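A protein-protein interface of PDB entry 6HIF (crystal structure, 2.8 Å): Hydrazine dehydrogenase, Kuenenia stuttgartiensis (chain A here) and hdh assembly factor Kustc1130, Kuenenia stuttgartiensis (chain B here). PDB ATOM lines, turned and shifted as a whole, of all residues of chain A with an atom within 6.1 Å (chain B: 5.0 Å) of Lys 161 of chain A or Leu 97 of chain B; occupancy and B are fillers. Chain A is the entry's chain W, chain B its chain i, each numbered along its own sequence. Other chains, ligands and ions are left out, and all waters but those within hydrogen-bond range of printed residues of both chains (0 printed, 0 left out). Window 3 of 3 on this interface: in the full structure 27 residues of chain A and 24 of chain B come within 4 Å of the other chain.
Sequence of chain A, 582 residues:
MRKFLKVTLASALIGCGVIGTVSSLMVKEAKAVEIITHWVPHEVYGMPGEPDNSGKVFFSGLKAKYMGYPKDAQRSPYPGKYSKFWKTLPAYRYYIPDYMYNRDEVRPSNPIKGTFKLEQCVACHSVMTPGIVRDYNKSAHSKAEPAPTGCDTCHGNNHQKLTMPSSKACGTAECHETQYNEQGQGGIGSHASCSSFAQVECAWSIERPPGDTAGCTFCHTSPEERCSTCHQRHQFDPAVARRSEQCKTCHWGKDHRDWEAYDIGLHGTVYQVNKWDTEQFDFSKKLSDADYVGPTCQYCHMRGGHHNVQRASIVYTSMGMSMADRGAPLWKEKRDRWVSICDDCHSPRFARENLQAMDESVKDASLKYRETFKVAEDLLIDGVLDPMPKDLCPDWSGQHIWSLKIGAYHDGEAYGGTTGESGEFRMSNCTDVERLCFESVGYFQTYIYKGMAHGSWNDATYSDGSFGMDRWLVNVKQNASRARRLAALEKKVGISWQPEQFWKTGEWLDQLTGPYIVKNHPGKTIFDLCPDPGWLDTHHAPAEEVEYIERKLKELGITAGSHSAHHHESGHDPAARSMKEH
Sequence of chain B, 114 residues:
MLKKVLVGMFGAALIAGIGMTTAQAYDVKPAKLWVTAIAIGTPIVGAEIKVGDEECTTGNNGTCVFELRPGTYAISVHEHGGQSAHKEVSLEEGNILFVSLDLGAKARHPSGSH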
ATOM      1  N   ASP A 104       6.721  18.914   3.642  1.00  0.00           N
ATOM      2  CA  ASP A 104       7.858  19.817   3.521  1.00  0.00           C
ATOM      3  C   ASP A 104       9.170  19.079   3.786  1.00  0.00           C
ATOM      4  O   ASP A 104      10.201  19.418   3.210  1.00  0.00           O
ATOM      5  CB  ASP A 104       7.720  21.027   4.448  1.00  0.00           C
ATOM      6  CG  ASP A 104       6.920  22.169   3.850  1.00  0.00           C
ATOM      7  OD1 ASP A 104       5.862  21.894   3.255  1.00  0.00           O
ATOM      8  OD2 ASP A 104       7.364  23.324   3.982  1.00  0.00           O
ATOM      9  N   ARG A 107       9.639  16.793   0.289  1.00  0.00           N
ATOM     10  CA  ARG A 107       9.579  17.397  -1.037  1.00  0.00           C
ATOM     11  C   ARG A 107      10.984  17.525  -1.624  1.00  0.00           C
ATOM     12  O   ARG A 107      11.876  18.074  -0.982  1.00  0.00           O
ATOM     13  CB  ARG A 107       8.896  18.767  -0.976  1.00  0.00           C
ATOM     14  CG  ARG A 107       8.866  19.500  -2.310  1.00  0.00           C
ATOM     15  CD  ARG A 107       8.403  20.939  -2.210  1.00  0.00           C
ATOM     16  NE  ARG A 107       6.966  21.043  -1.990  1.00  0.00           N
ATOM     17  CZ  ARG A 107       6.390  21.298  -0.819  1.00  0.00           C
ATOM     18  NH1 ARG A 107       7.126  21.490   0.262  1.00  0.00           N
ATOM     19  NH2 ARG A 107       5.075  21.367  -0.734  1.00  0.00           N
ATOM     20  N   HIS A 155      -0.652  21.719  -9.074  1.00  0.00           N
ATOM     21  CA  HIS A 155       0.740  21.556  -8.679  1.00  0.00           C
ATOM     22  C   HIS A 155       1.207  22.655  -7.728  1.00  0.00           C
ATOM     23  O   HIS A 155       2.181  22.459  -7.004  1.00  0.00           O
ATOM     24  CB  HIS A 155       1.657  21.463  -9.904  1.00  0.00           C
ATOM     25  CG  HIS A 155       1.518  20.192 -10.667  1.00  0.00           C
ATOM     26  ND1 HIS A 155       1.923  18.977 -10.150  1.00  0.00           N
ATOM     27  CD2 HIS A 155       1.038  19.939 -11.903  1.00  0.00           C
ATOM     28  CE1 HIS A 155       1.689  18.028 -11.033  1.00  0.00           C
ATOM     29  NE2 HIS A 155       1.148  18.594 -12.114  1.00  0.00           N
ATOM     30  N   GLY A 156       0.530  23.808  -7.750  1.00  0.00           N
ATOM     31  CA  GLY A 156       0.919  24.937  -6.918  1.00  0.00           C
ATOM     32  C   GLY A 156       1.631  26.020  -7.725  1.00  0.00           C
ATOM     33  O   GLY A 156       2.028  25.781  -8.864  1.00  0.00           O
ATOM     34  N   ASN A 157       1.789  27.201  -7.112  1.00  0.00           N
ATOM     35  CA  ASN A 157       2.328  28.378  -7.775  1.00  0.00           C
ATOM     36  C   ASN A 157       3.826  28.491  -7.516  1.00  0.00           C
ATOM     37  O   ASN A 157       4.574  28.913  -8.394  1.00  0.00           O
ATOM     38  CB  ASN A 157       1.626  29.660  -7.329  1.00  0.00           C
ATOM     39  CG  ASN A 157       0.305  29.876  -8.033  1.00  0.00           C
ATOM     40  OD1 ASN A 157      -0.743  29.872  -7.397  1.00  0.00           O
ATOM     41  ND2 ASN A 157       0.340  30.054  -9.344  1.00  0.00           N
ATOM     42  N   ASN A 158       4.240  28.124  -6.300  1.00  0.00           N
ATOM     43  CA  ASN A 158       5.623  28.249  -5.876  1.00  0.00           C
ATOM     44  C   ASN A 158       6.417  27.055  -6.399  1.00  0.00           C
ATOM     45  O   ASN A 158       6.137  25.915  -6.036  1.00  0.00           O
ATOM     46  CB  ASN A 158       5.722  28.386  -4.355  1.00  0.00           C
ATOM     47  CG  ASN A 158       7.104  28.760  -3.864  1.00  0.00           C
ATOM     48  OD1 ASN A 158       8.091  28.667  -4.594  1.00  0.00           O
ATOM     49  ND2 ASN A 158       7.186  29.178  -2.612  1.00  0.00           N
ATOM     50  N   HIS A 159       7.421  27.333  -7.237  1.00  0.00           N
ATOM     51  CA  HIS A 159       8.178  26.276  -7.889  1.00  0.00           C
ATOM     52  C   HIS A 159       9.092  25.572  -6.889  1.00  0.00           C
ATOM     53  O   HIS A 159       9.591  24.481  -7.167  1.00  0.00           O
ATOM     54  CB  HIS A 159       8.934  26.810  -9.109  1.00  0.00           C
ATOM     55  CG  HIS A 159       9.017  25.807 -10.208  1.00  0.00           C
ATOM     56  ND1 HIS A 159      10.091  24.953 -10.354  1.00  0.00           N
ATOM     57  CD2 HIS A 159       8.150  25.495 -11.194  1.00  0.00           C
ATOM     58  CE1 HIS A 159       9.890  24.172 -11.397  1.00  0.00           C
ATOM     59  NE2 HIS A 159       8.706  24.486 -11.927  1.00  0.00           N
ATOM     60  N   GLN A 160       9.300  26.203  -5.728  1.00  0.00           N
ATOM     61  CA  GLN A 160      10.103  25.618  -4.667  1.00  0.00           C
ATOM     62  C   GLN A 160       9.210  24.817  -3.722  1.00  0.00           C
ATOM     63  O   GLN A 160       9.706  24.073  -2.877  1.00  0.00           O
ATOM     64  CB  GLN A 160      10.905  26.699  -3.939  1.00  0.00           C
ATOM     65  CG  GLN A 160      12.070  27.248  -4.751  1.00  0.00           C
ATOM     66  CD  GLN A 160      13.062  26.181  -5.151  1.00  0.00           C
ATOM     67  OE1 GLN A 160      13.774  25.623  -4.322  1.00  0.00           O
ATOM     68  NE2 GLN A 160      13.122  25.888  -6.441  1.00  0.00           N
ATOM     69  N   LYS A 161       7.889  24.970  -3.884  1.00  0.00           N
ATOM     70  CA  LYS A 161       6.922  24.278  -3.048  1.00  0.00           C
ATOM     71  C   LYS A 161       5.872  23.597  -3.922  1.00  0.00           C
ATOM     72  O   LYS A 161       4.676  23.686  -3.655  1.00  0.00           O
ATOM     73  CB  LYS A 161       6.319  25.237  -2.015  1.00  0.00           C
ATOM     74  CG  LYS A 161       7.223  25.549  -0.829  1.00  0.00           C
ATOM     75  CD  LYS A 161       6.656  26.584   0.117  1.00  0.00           C
ATOM     76  CE  LYS A 161       7.496  26.754   1.364  1.00  0.00           C
ATOM     77  NZ  LYS A 161       7.041  27.910   2.172  1.00  0.00           N
ATOM     78  N   LEU A 162       6.343  22.904  -4.965  1.00  0.00           N
ATOM     79  CA  LEU A 162       5.474  22.167  -5.868  1.00  0.00           C
ATOM     80  C   LEU A 162       4.923  20.935  -5.152  1.00  0.00           C
ATOM     81  O   LEU A 162       5.565  20.393  -4.253  1.00  0.00           O
ATOM     82  CB  LEU A 162       6.270  21.760  -7.116  1.00  0.00           C
ATOM     83  CG  LEU A 162       6.591  22.879  -8.108  1.00  0.00           C
ATOM     84  CD1 LEU A 162       7.571  22.395  -9.166  1.00  0.00           C
ATOM     85  CD2 LEU A 162       5.325  23.410  -8.765  1.00  0.00           C
ATOM     86  N   THR A 163       3.725  20.507  -5.566  1.00  0.00           N
ATOM     87  CA  THR A 163       3.102  19.312  -5.023  1.00  0.00           C
ATOM     88  C   THR A 163       2.588  18.437  -6.161  1.00  0.00           C
ATOM     89  O   THR A 163       2.299  18.931  -7.246  1.00  0.00           O
ATOM     90  CB  THR A 163       1.973  19.656  -4.043  1.00  0.00           C
ATOM     91  OG1 THR A 163       1.030  20.485  -4.721  1.00  0.00           O
ATOM     92  CG2 THR A 163       2.463  20.349  -2.791  1.00  0.00           C
ATOM     93  N   LYS B  32      -5.153  30.207  -2.556  1.00  0.00           N
ATOM     94  CA  LYS B  32      -5.848  28.949  -2.336  1.00  0.00           C
ATOM     95  C   LYS B  32      -4.913  27.998  -1.594  1.00  0.00           C
ATOM     96  O   LYS B  32      -3.817  27.707  -2.069  1.00  0.00           O
ATOM     97  CB  LYS B  32      -6.351  28.368  -3.662  1.00  0.00           C
ATOM     98  CG  LYS B  32      -7.766  27.806  -3.627  1.00  0.00           C
ATOM     99  CD  LYS B  32      -8.236  27.227  -4.948  1.00  0.00           C
ATOM    100  CE  LYS B  32      -9.644  26.666  -4.889  1.00  0.00           C
ATOM    101  NZ  LYS B  32      -9.874  25.614  -5.909  1.00  0.00           N
ATOM    102  N   LEU B  33      -5.357  27.536  -0.417  1.00  0.00           N
ATOM    103  CA  LEU B  33      -4.563  26.664   0.434  1.00  0.00           C
ATOM    104  C   LEU B  33      -5.284  25.333   0.629  1.00  0.00           C
ATOM    105  O   LEU B  33      -6.401  25.291   1.141  1.00  0.00           O
ATOM    106  CB  LEU B  33      -4.311  27.356   1.779  1.00  0.00           C
ATOM    107  CG  LEU B  33      -3.533  26.539   2.812  1.00  0.00           C
ATOM    108  CD1 LEU B  33      -2.052  26.480   2.463  1.00  0.00           C
ATOM    109  CD2 LEU B  33      -3.723  27.117   4.204  1.00  0.00           C
ATOM    110  N   TRP B  34      -4.616  24.255   0.207  1.00  0.00           N
ATOM    111  CA  TRP B  34      -5.061  22.893   0.448  1.00  0.00           C
ATOM    112  C   TRP B  34      -4.323  22.355   1.670  1.00  0.00           C
ATOM    113  O   TRP B  34      -3.100  22.455   1.748  1.00  0.00           O
ATOM    114  CB  TRP B  34      -4.778  22.014  -0.777  1.00  0.00           C
ATOM    115  CG  TRP B  34      -5.383  22.472  -2.070  1.00  0.00           C
ATOM    116  CD1 TRP B  34      -5.157  23.650  -2.722  1.00  0.00           C
ATOM    117  CD2 TRP B  34      -6.288  21.725  -2.901  1.00  0.00           C
ATOM    118  NE1 TRP B  34      -5.874  23.698  -3.887  1.00  0.00           N
ATOM    119  CE2 TRP B  34      -6.575  22.530  -4.026  1.00  0.00           C
ATOM    120  CE3 TRP B  34      -6.885  20.463  -2.804  1.00  0.00           C
ATOM    121  CZ2 TRP B  34      -7.437  22.110  -5.039  1.00  0.00           C
ATOM    122  CZ3 TRP B  34      -7.736  20.049  -3.806  1.00  0.00           C
ATOM    123  CH2 TRP B  34      -8.006  20.863  -4.907  1.00  0.00           C
ATOM    124  N   VAL B  89       2.252  29.670   7.640  1.00  0.00           N
ATOM    125  CA  VAL B  89       2.365  29.842   6.200  1.00  0.00           C
ATOM    126  C   VAL B  89       2.086  31.302   5.839  1.00  0.00           C
ATOM    127  O   VAL B  89       1.095  31.876   6.287  1.00  0.00           O
ATOM    128  CB  VAL B  89       1.430  28.865   5.455  1.00  0.00           C
ATOM    129  CG1 VAL B  89       1.058  29.348   4.064  1.00  0.00           C
ATOM    130  CG2 VAL B  89       2.011  27.461   5.389  1.00  0.00           C
ATOM    131  N   LEU B  91       1.149  33.672   2.780  1.00  0.00           N
ATOM    132  CA  LEU B  91       0.537  33.589   1.463  1.00  0.00           C
ATOM    133  C   LEU B  91       0.517  34.966   0.805  1.00  0.00           C
ATOM    134  O   LEU B  91       0.123  35.954   1.422  1.00  0.00           O
ATOM    135  CB  LEU B  91      -0.881  33.021   1.598  1.00  0.00           C
ATOM    136  CG  LEU B  91      -0.975  31.543   1.970  1.00  0.00           C
ATOM    137  CD1 LEU B  91      -2.406  31.162   2.313  1.00  0.00           C
ATOM    138  CD2 LEU B  91      -0.444  30.655   0.854  1.00  0.00           C
ATOM    139  N   ASN B  95      -1.641  32.968  -4.680  1.00  0.00           N
ATOM    140  CA  ASN B  95      -0.792  31.821  -4.399  1.00  0.00           C
ATOM    141  C   ASN B  95      -1.648  30.560  -4.332  1.00  0.00           C
ATOM    142  O   ASN B  95      -2.785  30.600  -3.866  1.00  0.00           O
ATOM    143  CB  ASN B  95      -0.017  31.989  -3.088  1.00  0.00           C
ATOM    144  CG  ASN B  95       1.231  32.839  -3.218  1.00  0.00           C
ATOM    145  OD1 ASN B  95       1.415  33.547  -4.205  1.00  0.00           O
ATOM    146  ND2 ASN B  95       2.097  32.775  -2.219  1.00  0.00           N
ATOM    147  N   ILE B  96      -1.089  29.444  -4.812  1.00  0.00           N
ATOM    148  CA  ILE B  96      -1.686  28.133  -4.609  1.00  0.00           C
ATOM    149  C   ILE B  96      -0.643  27.248  -3.933  1.00  0.00           C
ATOM    150  O   ILE B  96       0.454  27.059  -4.459  1.00  0.00           O
ATOM    151  CB  ILE B  96      -2.224  27.524  -5.923  1.00  0.00           C
ATOM    152  CG1 ILE B  96      -3.339  28.377  -6.537  1.00  0.00           C
ATOM    153  CG2 ILE B  96      -2.684  26.090  -5.701  1.00  0.00           C
ATOM    154  CD1 ILE B  96      -3.549  28.160  -8.021  1.00  0.00           C
ATOM    155  N   LEU B  97      -0.998  26.736  -2.750  1.00  0.00           N
ATOM    156  CA  LEU B  97      -0.105  25.901  -1.965  1.00  0.00           C
ATOM    157  C   LEU B  97      -0.877  24.706  -1.414  1.00  0.00           C
ATOM    158  O   LEU B  97      -1.959  24.864  -0.849  1.00  0.00           O
ATOM    159  CB  LEU B  97       0.498  26.736  -0.829  1.00  0.00           C
ATOM    160  CG  LEU B  97       1.553  26.031   0.026  1.00  0.00           C
ATOM    161  CD1 LEU B  97       2.865  25.888  -0.734  1.00  0.00           C
ATOM    162  CD2 LEU B  97       1.774  26.779   1.330  1.00  0.00           C
ATOM    163  N   PHE B  98      -0.300  23.515  -1.603  1.00  0.00           N
ATOM    164  CA  PHE B  98      -0.777  22.304  -0.959  1.00  0.00           C
ATOM    165  C   PHE B  98       0.109  22.025   0.251  1.00  0.00           C
ATOM    166  O   PHE B  98       1.334  22.001   0.134  1.00  0.00           O
ATOM    167  CB  PHE B  98      -0.751  21.127  -1.936  1.00  0.00           C
ATOM    168  CG  PHE B  98      -1.744  21.179  -3.072  1.00  0.00           C
ATOM    169  CD1 PHE B  98      -1.686  22.180  -4.033  1.00  0.00           C
ATOM    170  CD2 PHE B  98      -2.720  20.202  -3.200  1.00  0.00           C
ATOM    171  CE1 PHE B  98      -2.596  22.215  -5.079  1.00  0.00           C
ATOM    172  CE2 PHE B  98      -3.627  20.234  -4.250  1.00  0.00           C
ATOM    173  CZ  PHE B  98      -3.565  21.241  -5.187  1.00  0.00           C
ATOM    174  N   VAL B  99      -0.527  21.841   1.413  1.00  0.00           N
ATOM    175  CA  VAL B  99       0.175  21.528   2.647  1.00  0.00           C
ATOM    176  C   VAL B  99      -0.252  20.135   3.103  1.00  0.00           C
ATOM    177  O   VAL B  99      -1.442  19.836   3.172  1.00  0.00           O
ATOM    178  CB  VAL B  99      -0.069  22.600   3.729  1.00  0.00           C
ATOM    179  CG1 VAL B  99       0.396  22.146   5.106  1.00  0.00           C
ATOM    180  CG2 VAL B  99       0.581  23.925   3.364  1.00  0.00           C
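Lys 161 of chain A touches just one residue of chain B: Leu 97. Of chain A, only Lys 161 comes within 4 Å of Leu 97 of chain B. Of the printed residues of chain A, Phe 98 of chain B touches Arg 107 (3.9 Å) and Thr 163 (3.3 Å). Printed residues of chain B within 4 Å of Thr 163 of chain A: Phe 98 (3.3 Å). Of the printed residues of chain B, Gly 156 of chain A touches Ile 96. Printed residues of chain A within 4 Å of Asn 95 of chain B: Asn 157 (3.3 Å). Leu 91 of chain B touches none of the printed residues of chain A.
Phe 98 of chain B touches Arg 107 of chain A. Gly 156 of chain A touches Ile 96 of chain B. C of Asn 95 of chain B touches OD1 of Asn 157 of chain A, 3.3 Å away. Leu 97 of chain B touches Lys 161 of chain A (CD1 to CB, 3.7 Å). OG1 of Thr 163 of chain A touches CD1 of Phe 98 of chain B, 3.3 Å away.
The side-chain amide oxygen (OD1) of Asn 157 of chain A sits at hydrogen-bond distance from the backbone NH (N) of Ile 96 of chain B (2.6 Å).
The backbone NH of Leu 97 of chain B is in hydrogen-bond range of the backbone carbonyl oxygen of Lys 32 of chain B (3.1 Å). O of Leu 162 of chain A sits at hydrogen-bond distance from NE of Arg 107 of chain A (2.7 Å). The side-chain carboxylate (OD1) of Asp 104 of chain A is in salt-bridge range of the guanidinium group (NH1) of Arg 107 of chain A (3.3 Å). N of Trp 34 of chain B sits at hydrogen-bond distance from O of Leu 97 of chain B (2.9 Å). The backbone NH of Thr 163 of chain A lies within hydrogen-bond range of the backbone carbonyl oxygen of His 155 of chain A, at 2.9 Å. The backbone carbonyl oxygen (O) of Asn 95 of chain B is in hydrogen-bond range of the backbone NH (N) of Lys 32 of chain B, at 2.7 Å.
Hydrophobic or aromatic side chains of chain B within 4 Å of the printed part of chain A: Ile 96, Leu 97 and Phe 98.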
